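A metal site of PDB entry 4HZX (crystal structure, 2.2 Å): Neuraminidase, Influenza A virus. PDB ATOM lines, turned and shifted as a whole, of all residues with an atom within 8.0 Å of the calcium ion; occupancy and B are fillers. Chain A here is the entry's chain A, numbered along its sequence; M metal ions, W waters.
Merely in contact with the calcium ion: Gly 266 (3.9 Å).
N of Lys 216 lies within hydrogen-bond range of OD1 of Asp 213 (3.0 Å).
OD2 of Asp 213 lies within hydrogen-bond range of OH of Tyr 235, 2.7 Å away.
OD1 of Asn 214 lies close to O of Pro 265, 3.2 Å away.
N of Asp 243 sits close to O of Ser 218, 3.3 Å away.
OD1 of Asp 243 is in hydrogen-bond range of N of Val 267 (2.9 Å).
OD1 of Asp 243 is in salt-bridge range of NH2 of Arg 220, 3.6 Å away.
The backbone NH (N) of Gly 266 lies close to the backbone carbonyl oxygen (O) of Thr 244 (3.5 Å).
The backbone carbonyl oxygen (O) of Gly 266 sits at hydrogen-bond distance from the guanidinium group (NH2) of Arg 212 (3.3 Å).
The calcium ion is bound by water W1 (2.4 Å), the backbone carbonyl oxygen (O) of Asp 213 (2.5 Å), the backbone carbonyl oxygen (O) of Gly 263 (2.5 Å), the backbone carbonyl oxygen (O) of Pro 265 (2.5 Å), the backbone carbonyl oxygen (O) of Gly 217 (2.6 Å) and the side-chain carboxylate (OD2) of Asp 243 (2.7 Å).
Water W1 lies within hydrogen-bond range of O of Asn 262 and O of Pro 245.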
ATOM      1  N   HIS A 195      11.941 -17.221 -25.920  1.00  0.00           N
ATOM      2  CA  HIS A 195      10.755 -18.004 -25.625  1.00  0.00           C
ATOM      3  C   HIS A 195      10.622 -18.177 -24.120  1.00  0.00           C
ATOM      4  O   HIS A 195      11.611 -18.393 -23.422  1.00  0.00           O
ATOM      5  CB  HIS A 195      10.803 -19.378 -26.311  1.00  0.00           C
ATOM      6  CG  HIS A 195       9.474 -20.052 -26.410  1.00  0.00           C
ATOM      7  ND1 HIS A 195       8.506 -19.662 -27.318  1.00  0.00           N
ATOM      8  CD2 HIS A 195       8.933 -21.067 -25.694  1.00  0.00           C
ATOM      9  CE1 HIS A 195       7.434 -20.428 -27.168  1.00  0.00           C
ATOM     10  NE2 HIS A 195       7.668 -21.290 -26.195  1.00  0.00           N
ATOM     11  N   CYS A 211      12.508 -19.802 -15.955  1.00  0.00           N
ATOM     12  CA  CYS A 211      11.397 -20.329 -16.743  1.00  0.00           C
ATOM     13  C   CYS A 211      11.786 -21.434 -17.716  1.00  0.00           C
ATOM     14  O   CYS A 211      12.846 -22.052 -17.597  1.00  0.00           O
ATOM     15  CB  CYS A 211      10.717 -19.175 -17.484  1.00  0.00           C
ATOM     16  SG  CYS A 211      10.524 -17.669 -16.478  1.00  0.00           S
ATOM     17  N   ARG A 212      10.900 -21.666 -18.678  1.00  0.00           N
ATOM     18  CA  ARG A 212      11.065 -22.714 -19.683  1.00  0.00           C
ATOM     19  C   ARG A 212      11.016 -22.122 -21.095  1.00  0.00           C
ATOM     20  O   ARG A 212      10.020 -21.522 -21.485  1.00  0.00           O
ATOM     21  CB  ARG A 212       9.971 -23.774 -19.522  1.00  0.00           C
ATOM     22  CG  ARG A 212       9.767 -24.706 -20.704  1.00  0.00           C
ATOM     23  CD  ARG A 212       8.656 -25.695 -20.397  1.00  0.00           C
ATOM     24  NE  ARG A 212       8.185 -26.424 -21.570  1.00  0.00           N
ATOM     25  CZ  ARG A 212       7.253 -27.375 -21.525  1.00  0.00           C
ATOM     26  NH1 ARG A 212       6.701 -27.716 -20.376  1.00  0.00           N
ATOM     27  NH2 ARG A 212       6.872 -27.992 -22.634  1.00  0.00           N
ATOM     28  N   ASP A 213      12.106 -22.281 -21.831  1.00  0.00           N
ATOM     29  CA  ASP A 213      12.139 -21.892 -23.237  1.00  0.00           C
ATOM     30  C   ASP A 213      11.787 -23.155 -23.998  1.00  0.00           C
ATOM     31  O   ASP A 213      12.517 -24.134 -23.947  1.00  0.00           O
ATOM     32  CB  ASP A 213      13.533 -21.386 -23.617  1.00  0.00           C
ATOM     33  CG  ASP A 213      13.694 -21.169 -25.106  1.00  0.00           C
ATOM     34  OD1 ASP A 213      13.169 -21.977 -25.900  1.00  0.00           O
ATOM     35  OD2 ASP A 213      14.342 -20.174 -25.491  1.00  0.00           O
ATOM     36  N   ASN A 214      10.656 -23.155 -24.705  1.00  0.00           N
ATOM     37  CA  ASN A 214      10.176 -24.374 -25.343  1.00  0.00           C
ATOM     38  C   ASN A 214      10.572 -24.464 -26.812  1.00  0.00           C
ATOM     39  O   ASN A 214      10.081 -25.323 -27.546  1.00  0.00           O
ATOM     40  CB  ASN A 214       8.652 -24.472 -25.211  1.00  0.00           C
ATOM     41  CG  ASN A 214       8.152 -25.905 -25.263  1.00  0.00           C
ATOM     42  OD1 ASN A 214       8.699 -26.773 -24.578  1.00  0.00           O
ATOM     43  ND2 ASN A 214       7.139 -26.153 -26.079  1.00  0.00           N
ATOM     44  N   TRP A 215      11.487 -23.596 -27.237  1.00  0.00           N
ATOM     45  CA  TRP A 215      11.749 -23.409 -28.661  1.00  0.00           C
ATOM     46  C   TRP A 215      13.216 -23.681 -29.046  1.00  0.00           C
ATOM     47  O   TRP A 215      13.520 -24.696 -29.682  1.00  0.00           O
ATOM     48  CB  TRP A 215      11.326 -21.996 -29.076  1.00  0.00           C
ATOM     49  CG  TRP A 215      11.494 -21.690 -30.538  1.00  0.00           C
ATOM     50  CD1 TRP A 215      11.634 -22.581 -31.568  1.00  0.00           C
ATOM     51  CD2 TRP A 215      11.558 -20.387 -31.129  1.00  0.00           C
ATOM     52  NE1 TRP A 215      11.768 -21.913 -32.758  1.00  0.00           N
ATOM     53  CE2 TRP A 215      11.727 -20.562 -32.524  1.00  0.00           C
ATOM     54  CE3 TRP A 215      11.482 -19.082 -30.621  1.00  0.00           C
ATOM     55  CZ2 TRP A 215      11.828 -19.482 -33.406  1.00  0.00           C
ATOM     56  CZ3 TRP A 215      11.575 -18.013 -31.501  1.00  0.00           C
ATOM     57  CH2 TRP A 215      11.747 -18.224 -32.875  1.00  0.00           C
ATOM     58  N   LYS A 216      14.115 -22.782 -28.664  1.00  0.00           N
ATOM     59  CA  LYS A 216      15.515 -22.891 -29.070  1.00  0.00           C
ATOM     60  C   LYS A 216      16.493 -23.063 -27.915  1.00  0.00           C
ATOM     61  O   LYS A 216      17.676 -23.301 -28.133  1.00  0.00           O
ATOM     62  CB  LYS A 216      15.928 -21.651 -29.877  1.00  0.00           C
ATOM     63  CG  LYS A 216      15.159 -21.444 -31.174  1.00  0.00           C
ATOM     64  CD  LYS A 216      15.402 -20.047 -31.737  1.00  0.00           C
ATOM     65  CE  LYS A 216      14.983 -18.962 -30.743  1.00  0.00           C
ATOM     66  NZ  LYS A 216      15.101 -17.580 -31.322  1.00  0.00           N
ATOM     67  N   GLY A 217      16.013 -22.945 -26.675  1.00  0.00           N
ATOM     68  CA  GLY A 217      16.924 -22.954 -25.541  1.00  0.00           C
ATOM     69  C   GLY A 217      16.870 -24.175 -24.650  1.00  0.00           C
ATOM     70  O   GLY A 217      15.818 -24.469 -24.068  1.00  0.00           O
ATOM     71  N   SER A 218      17.981 -24.887 -24.545  1.00  0.00           N
ATOM     72  CA  SER A 218      18.131 -25.962 -23.562  1.00  0.00           C
ATOM     73  C   SER A 218      18.569 -25.369 -22.223  1.00  0.00           C
ATOM     74  O   SER A 218      18.518 -26.033 -21.185  1.00  0.00           O
ATOM     75  CB  SER A 218      19.118 -27.030 -24.042  1.00  0.00           C
ATOM     76  OG  SER A 218      20.381 -26.468 -24.358  1.00  0.00           O
ATOM     77  N   ASN A 219      19.009 -24.121 -22.276  1.00  0.00           N
ATOM     78  CA  ASN A 219      19.220 -23.316 -21.077  1.00  0.00           C
ATOM     79  C   ASN A 219      17.913 -22.622 -20.704  1.00  0.00           C
ATOM     80  O   ASN A 219      17.024 -22.495 -21.542  1.00  0.00           O
ATOM     81  CB  ASN A 219      20.363 -22.307 -21.267  1.00  0.00           C
ATOM     82  CG  ASN A 219      20.234 -21.502 -22.558  1.00  0.00           C
ATOM     83  OD1 ASN A 219      19.576 -21.921 -23.505  1.00  0.00           O
ATOM     84  ND2 ASN A 219      20.879 -20.343 -22.597  1.00  0.00           N
ATOM     85  N   ARG A 220      17.804 -22.176 -19.456  1.00  0.00           N
ATOM     86  CA  ARG A 220      16.557 -21.574 -18.981  1.00  0.00           C
ATOM     87  C   ARG A 220      16.586 -20.051 -18.966  1.00  0.00           C
ATOM     88  O   ARG A 220      17.503 -19.450 -18.413  1.00  0.00           O
ATOM     89  CB  ARG A 220      16.202 -22.085 -17.571  1.00  0.00           C
ATOM     90  CG  ARG A 220      15.819 -23.563 -17.518  1.00  0.00           C
ATOM     91  CD  ARG A 220      15.036 -23.874 -16.254  1.00  0.00           C
ATOM     92  NE  ARG A 220      14.699 -25.298 -16.146  1.00  0.00           N
ATOM     93  CZ  ARG A 220      13.649 -25.864 -16.720  1.00  0.00           C
ATOM     94  NH1 ARG A 220      12.822 -25.142 -17.456  1.00  0.00           N
ATOM     95  NH2 ARG A 220      13.425 -27.160 -16.564  1.00  0.00           N
ATOM     96  N   PRO A 221      15.559 -19.414 -19.555  1.00  0.00           N
ATOM     97  CA  PRO A 221      15.423 -17.955 -19.544  1.00  0.00           C
ATOM     98  C   PRO A 221      15.060 -17.455 -18.151  1.00  0.00           C
ATOM     99  O   PRO A 221      14.428 -18.192 -17.407  1.00  0.00           O
ATOM    100  CB  PRO A 221      14.256 -17.699 -20.504  1.00  0.00           C
ATOM    101  CG  PRO A 221      13.445 -18.951 -20.436  1.00  0.00           C
ATOM    102  CD  PRO A 221      14.426 -20.075 -20.224  1.00  0.00           C
ATOM    103  N   TYR A 235      19.447 -15.552 -19.886  1.00  0.00           N
ATOM    104  CA  TYR A 235      19.392 -16.997 -19.702  1.00  0.00           C
ATOM    105  C   TYR A 235      20.430 -17.365 -18.650  1.00  0.00           C
ATOM    106  O   TYR A 235      21.432 -16.658 -18.492  1.00  0.00           O
ATOM    107  CB  TYR A 235      19.702 -17.747 -21.009  1.00  0.00           C
ATOM    108  CG  TYR A 235      18.554 -17.769 -21.997  1.00  0.00           C
ATOM    109  CD1 TYR A 235      18.266 -16.657 -22.779  1.00  0.00           C
ATOM    110  CD2 TYR A 235      17.770 -18.907 -22.157  1.00  0.00           C
ATOM    111  CE1 TYR A 235      17.217 -16.680 -23.695  1.00  0.00           C
ATOM    112  CE2 TYR A 235      16.721 -18.936 -23.061  1.00  0.00           C
ATOM    113  CZ  TYR A 235      16.450 -17.816 -23.822  1.00  0.00           C
ATOM    114  OH  TYR A 235      15.416 -17.839 -24.721  1.00  0.00           O
ATOM    115  N   SER A 242      19.789 -27.056 -17.667  1.00  0.00           N
ATOM    116  CA  SER A 242      18.819 -27.634 -16.734  1.00  0.00           C
ATOM    117  C   SER A 242      17.408 -27.846 -17.293  1.00  0.00           C
ATOM    118  O   SER A 242      16.475 -28.134 -16.553  1.00  0.00           O
ATOM    119  CB  SER A 242      18.741 -26.795 -15.449  1.00  0.00           C
ATOM    120  OG  SER A 242      18.339 -25.465 -15.724  1.00  0.00           O
ATOM    121  N   ASP A 243      17.242 -27.721 -18.606  1.00  0.00           N
ATOM    122  CA  ASP A 243      15.973 -28.075 -19.222  1.00  0.00           C
ATOM    123  C   ASP A 243      16.000 -29.542 -19.636  1.00  0.00           C
ATOM    124  O   ASP A 243      17.044 -30.193 -19.577  1.00  0.00           O
ATOM    125  CB  ASP A 243      15.681 -27.190 -20.442  1.00  0.00           C
ATOM    126  CG  ASP A 243      14.192 -27.049 -20.719  1.00  0.00           C
ATOM    127  OD1 ASP A 243      13.378 -27.787 -20.122  1.00  0.00           O
ATOM    128  OD2 ASP A 243      13.825 -26.198 -21.551  1.00  0.00           O
ATOM    129  N   THR A 244      14.853 -30.057 -20.067  1.00  0.00           N
ATOM    130  CA  THR A 244      14.756 -31.386 -20.646  1.00  0.00           C
ATOM    131  C   THR A 244      13.871 -31.287 -21.883  1.00  0.00           C
ATOM    132  O   THR A 244      12.714 -30.882 -21.781  1.00  0.00           O
ATOM    133  CB  THR A 244      14.114 -32.398 -19.660  1.00  0.00           C
ATOM    134  OG1 THR A 244      14.769 -32.301 -18.392  1.00  0.00           O
ATOM    135  CG2 THR A 244      14.232 -33.817 -20.185  1.00  0.00           C
ATOM    136  N   PRO A 245      14.395 -31.660 -23.057  1.00  0.00           N
ATOM    137  CA  PRO A 245      15.717 -32.241 -23.325  1.00  0.00           C
ATOM    138  C   PRO A 245      16.834 -31.210 -23.218  1.00  0.00           C
ATOM    139  O   PRO A 245      16.560 -30.023 -23.159  1.00  0.00           O
ATOM    140  CB  PRO A 245      15.593 -32.722 -24.771  1.00  0.00           C
ATOM    141  CG  PRO A 245      14.624 -31.777 -25.387  1.00  0.00           C
ATOM    142  CD  PRO A 245      13.622 -31.459 -24.302  1.00  0.00           C
ATOM    143  N   ARG A 246      18.077 -31.685 -23.181  1.00  0.00           N
ATOM    144  CA  ARG A 246      19.243 -30.806 -23.128  1.00  0.00           C
ATOM    145  C   ARG A 246      20.476 -31.596 -23.556  1.00  0.00           C
ATOM    146  O   ARG A 246      20.440 -32.831 -23.584  1.00  0.00           O
ATOM    147  CB  ARG A 246      19.456 -30.274 -21.718  1.00  0.00           C
ATOM    148  CG  ARG A 246      19.887 -31.344 -20.724  1.00  0.00           C
ATOM    149  CD  ARG A 246      20.124 -30.787 -19.324  1.00  0.00           C
ATOM    150  NE  ARG A 246      20.486 -31.851 -18.401  1.00  0.00           N
ATOM    151  CZ  ARG A 246      19.606 -32.590 -17.723  1.00  0.00           C
ATOM    152  NH1 ARG A 246      20.025 -33.535 -16.903  1.00  0.00           N
ATOM    153  NH2 ARG A 246      18.300 -32.379 -17.870  1.00  0.00           N
ATOM    154  N   SER A 259      20.485 -21.537 -26.201  1.00  0.00           N
ATOM    155  CA  SER A 259      21.642 -22.328 -26.604  1.00  0.00           C
ATOM    156  C   SER A 259      21.599 -22.706 -28.090  1.00  0.00           C
ATOM    157  O   SER A 259      22.644 -22.834 -28.726  1.00  0.00           O
ATOM    158  CB  SER A 259      21.743 -23.593 -25.763  1.00  0.00           C
ATOM    159  OG  SER A 259      20.709 -24.508 -26.097  1.00  0.00           O
ATOM    160  N   VAL A 261      20.715 -25.573 -29.066  1.00  0.00           N
ATOM    161  CA  VAL A 261      20.993 -27.005 -29.126  1.00  0.00           C
ATOM    162  C   VAL A 261      19.989 -27.763 -28.255  1.00  0.00           C
ATOM    163  O   VAL A 261      19.735 -27.384 -27.111  1.00  0.00           O
ATOM    164  CB  VAL A 261      22.443 -27.330 -28.678  1.00  0.00           C
ATOM    165  CG1 VAL A 261      23.436 -26.927 -29.760  1.00  0.00           C
ATOM    166  CG2 VAL A 261      22.771 -26.616 -27.375  1.00  0.00           C
ATOM    167  N   ASN A 262      19.419 -28.846 -28.799  1.00  0.00           N
ATOM    168  CA  ASN A 262      18.368 -29.588 -28.107  1.00  0.00           C
ATOM    169  C   ASN A 262      17.323 -28.625 -27.548  1.00  0.00           C
ATOM    170  O   ASN A 262      16.858 -28.776 -26.412  1.00  0.00           O
ATOM    171  CB  ASN A 262      18.955 -30.452 -26.988  1.00  0.00           C
ATOM    172  CG  ASN A 262      20.003 -31.426 -27.488  1.00  0.00           C
ATOM    173  OD1 ASN A 262      19.672 -32.455 -28.075  1.00  0.00           O
ATOM    174  ND2 ASN A 262      21.268 -31.103 -27.264  1.00  0.00           N
ATOM    175  N   GLY A 263      16.960 -27.639 -28.353  1.00  0.00           N
ATOM    176  CA  GLY A 263      16.148 -26.522 -27.910  1.00  0.00           C
ATOM    177  C   GLY A 263      14.700 -26.814 -27.562  1.00  0.00           C
ATOM    178  O   GLY A 263      14.140 -26.151 -26.703  1.00  0.00           O
ATOM    179  N   GLY A 264      14.080 -27.764 -28.242  1.00  0.00           N
ATOM    180  CA  GLY A 264      12.679 -28.066 -28.014  1.00  0.00           C
ATOM    181  C   GLY A 264      12.445 -29.546 -27.776  1.00  0.00           C
ATOM    182  O   GLY A 264      13.179 -30.379 -28.309  1.00  0.00           O
ATOM    183  N   PRO A 265      11.417 -29.888 -26.977  1.00  0.00           N
ATOM    184  CA  PRO A 265      10.498 -28.935 -26.335  1.00  0.00           C
ATOM    185  C   PRO A 265      11.035 -28.400 -25.004  1.00  0.00           C
ATOM    186  O   PRO A 265      11.785 -27.441 -25.011  1.00  0.00           O
ATOM    187  CB  PRO A 265       9.223 -29.769 -26.109  1.00  0.00           C
ATOM    188  CG  PRO A 265       9.689 -31.217 -26.114  1.00  0.00           C
ATOM    189  CD  PRO A 265      11.119 -31.280 -26.590  1.00  0.00           C
ATOM    190  N   GLY A 266      10.673 -29.024 -23.886  1.00  0.00           N
ATOM    191  CA  GLY A 266      11.127 -28.557 -22.594  1.00  0.00           C
ATOM    192  C   GLY A 266      10.286 -29.092 -21.450  1.00  0.00           C
ATOM    193  O   GLY A 266       9.363 -29.883 -21.647  1.00  0.00           O
ATOM    194  N   VAL A 267      10.609 -28.655 -20.231  1.00  0.00           N
ATOM    195  CA  VAL A 267       9.863 -29.022 -19.040  1.00  0.00           C
ATOM    196  C   VAL A 267       9.932 -27.874 -18.035  1.00  0.00           C
ATOM    197  O   VAL A 267      10.942 -27.175 -17.946  1.00  0.00           O
ATOM    198  CB  VAL A 267      10.419 -30.312 -18.392  1.00  0.00           C
ATOM    199  CG1 VAL A 267      11.723 -30.029 -17.662  1.00  0.00           C
ATOM    200  CG2 VAL A 267       9.407 -30.946 -17.451  1.00  0.00           C
HETATM  201 CA    CA M   1      13.835 -26.219 -24.209  1.00  0.00          CA
HETATM  202  O   HOH W   1      15.330 -28.117 -24.423  1.00  0.00           O
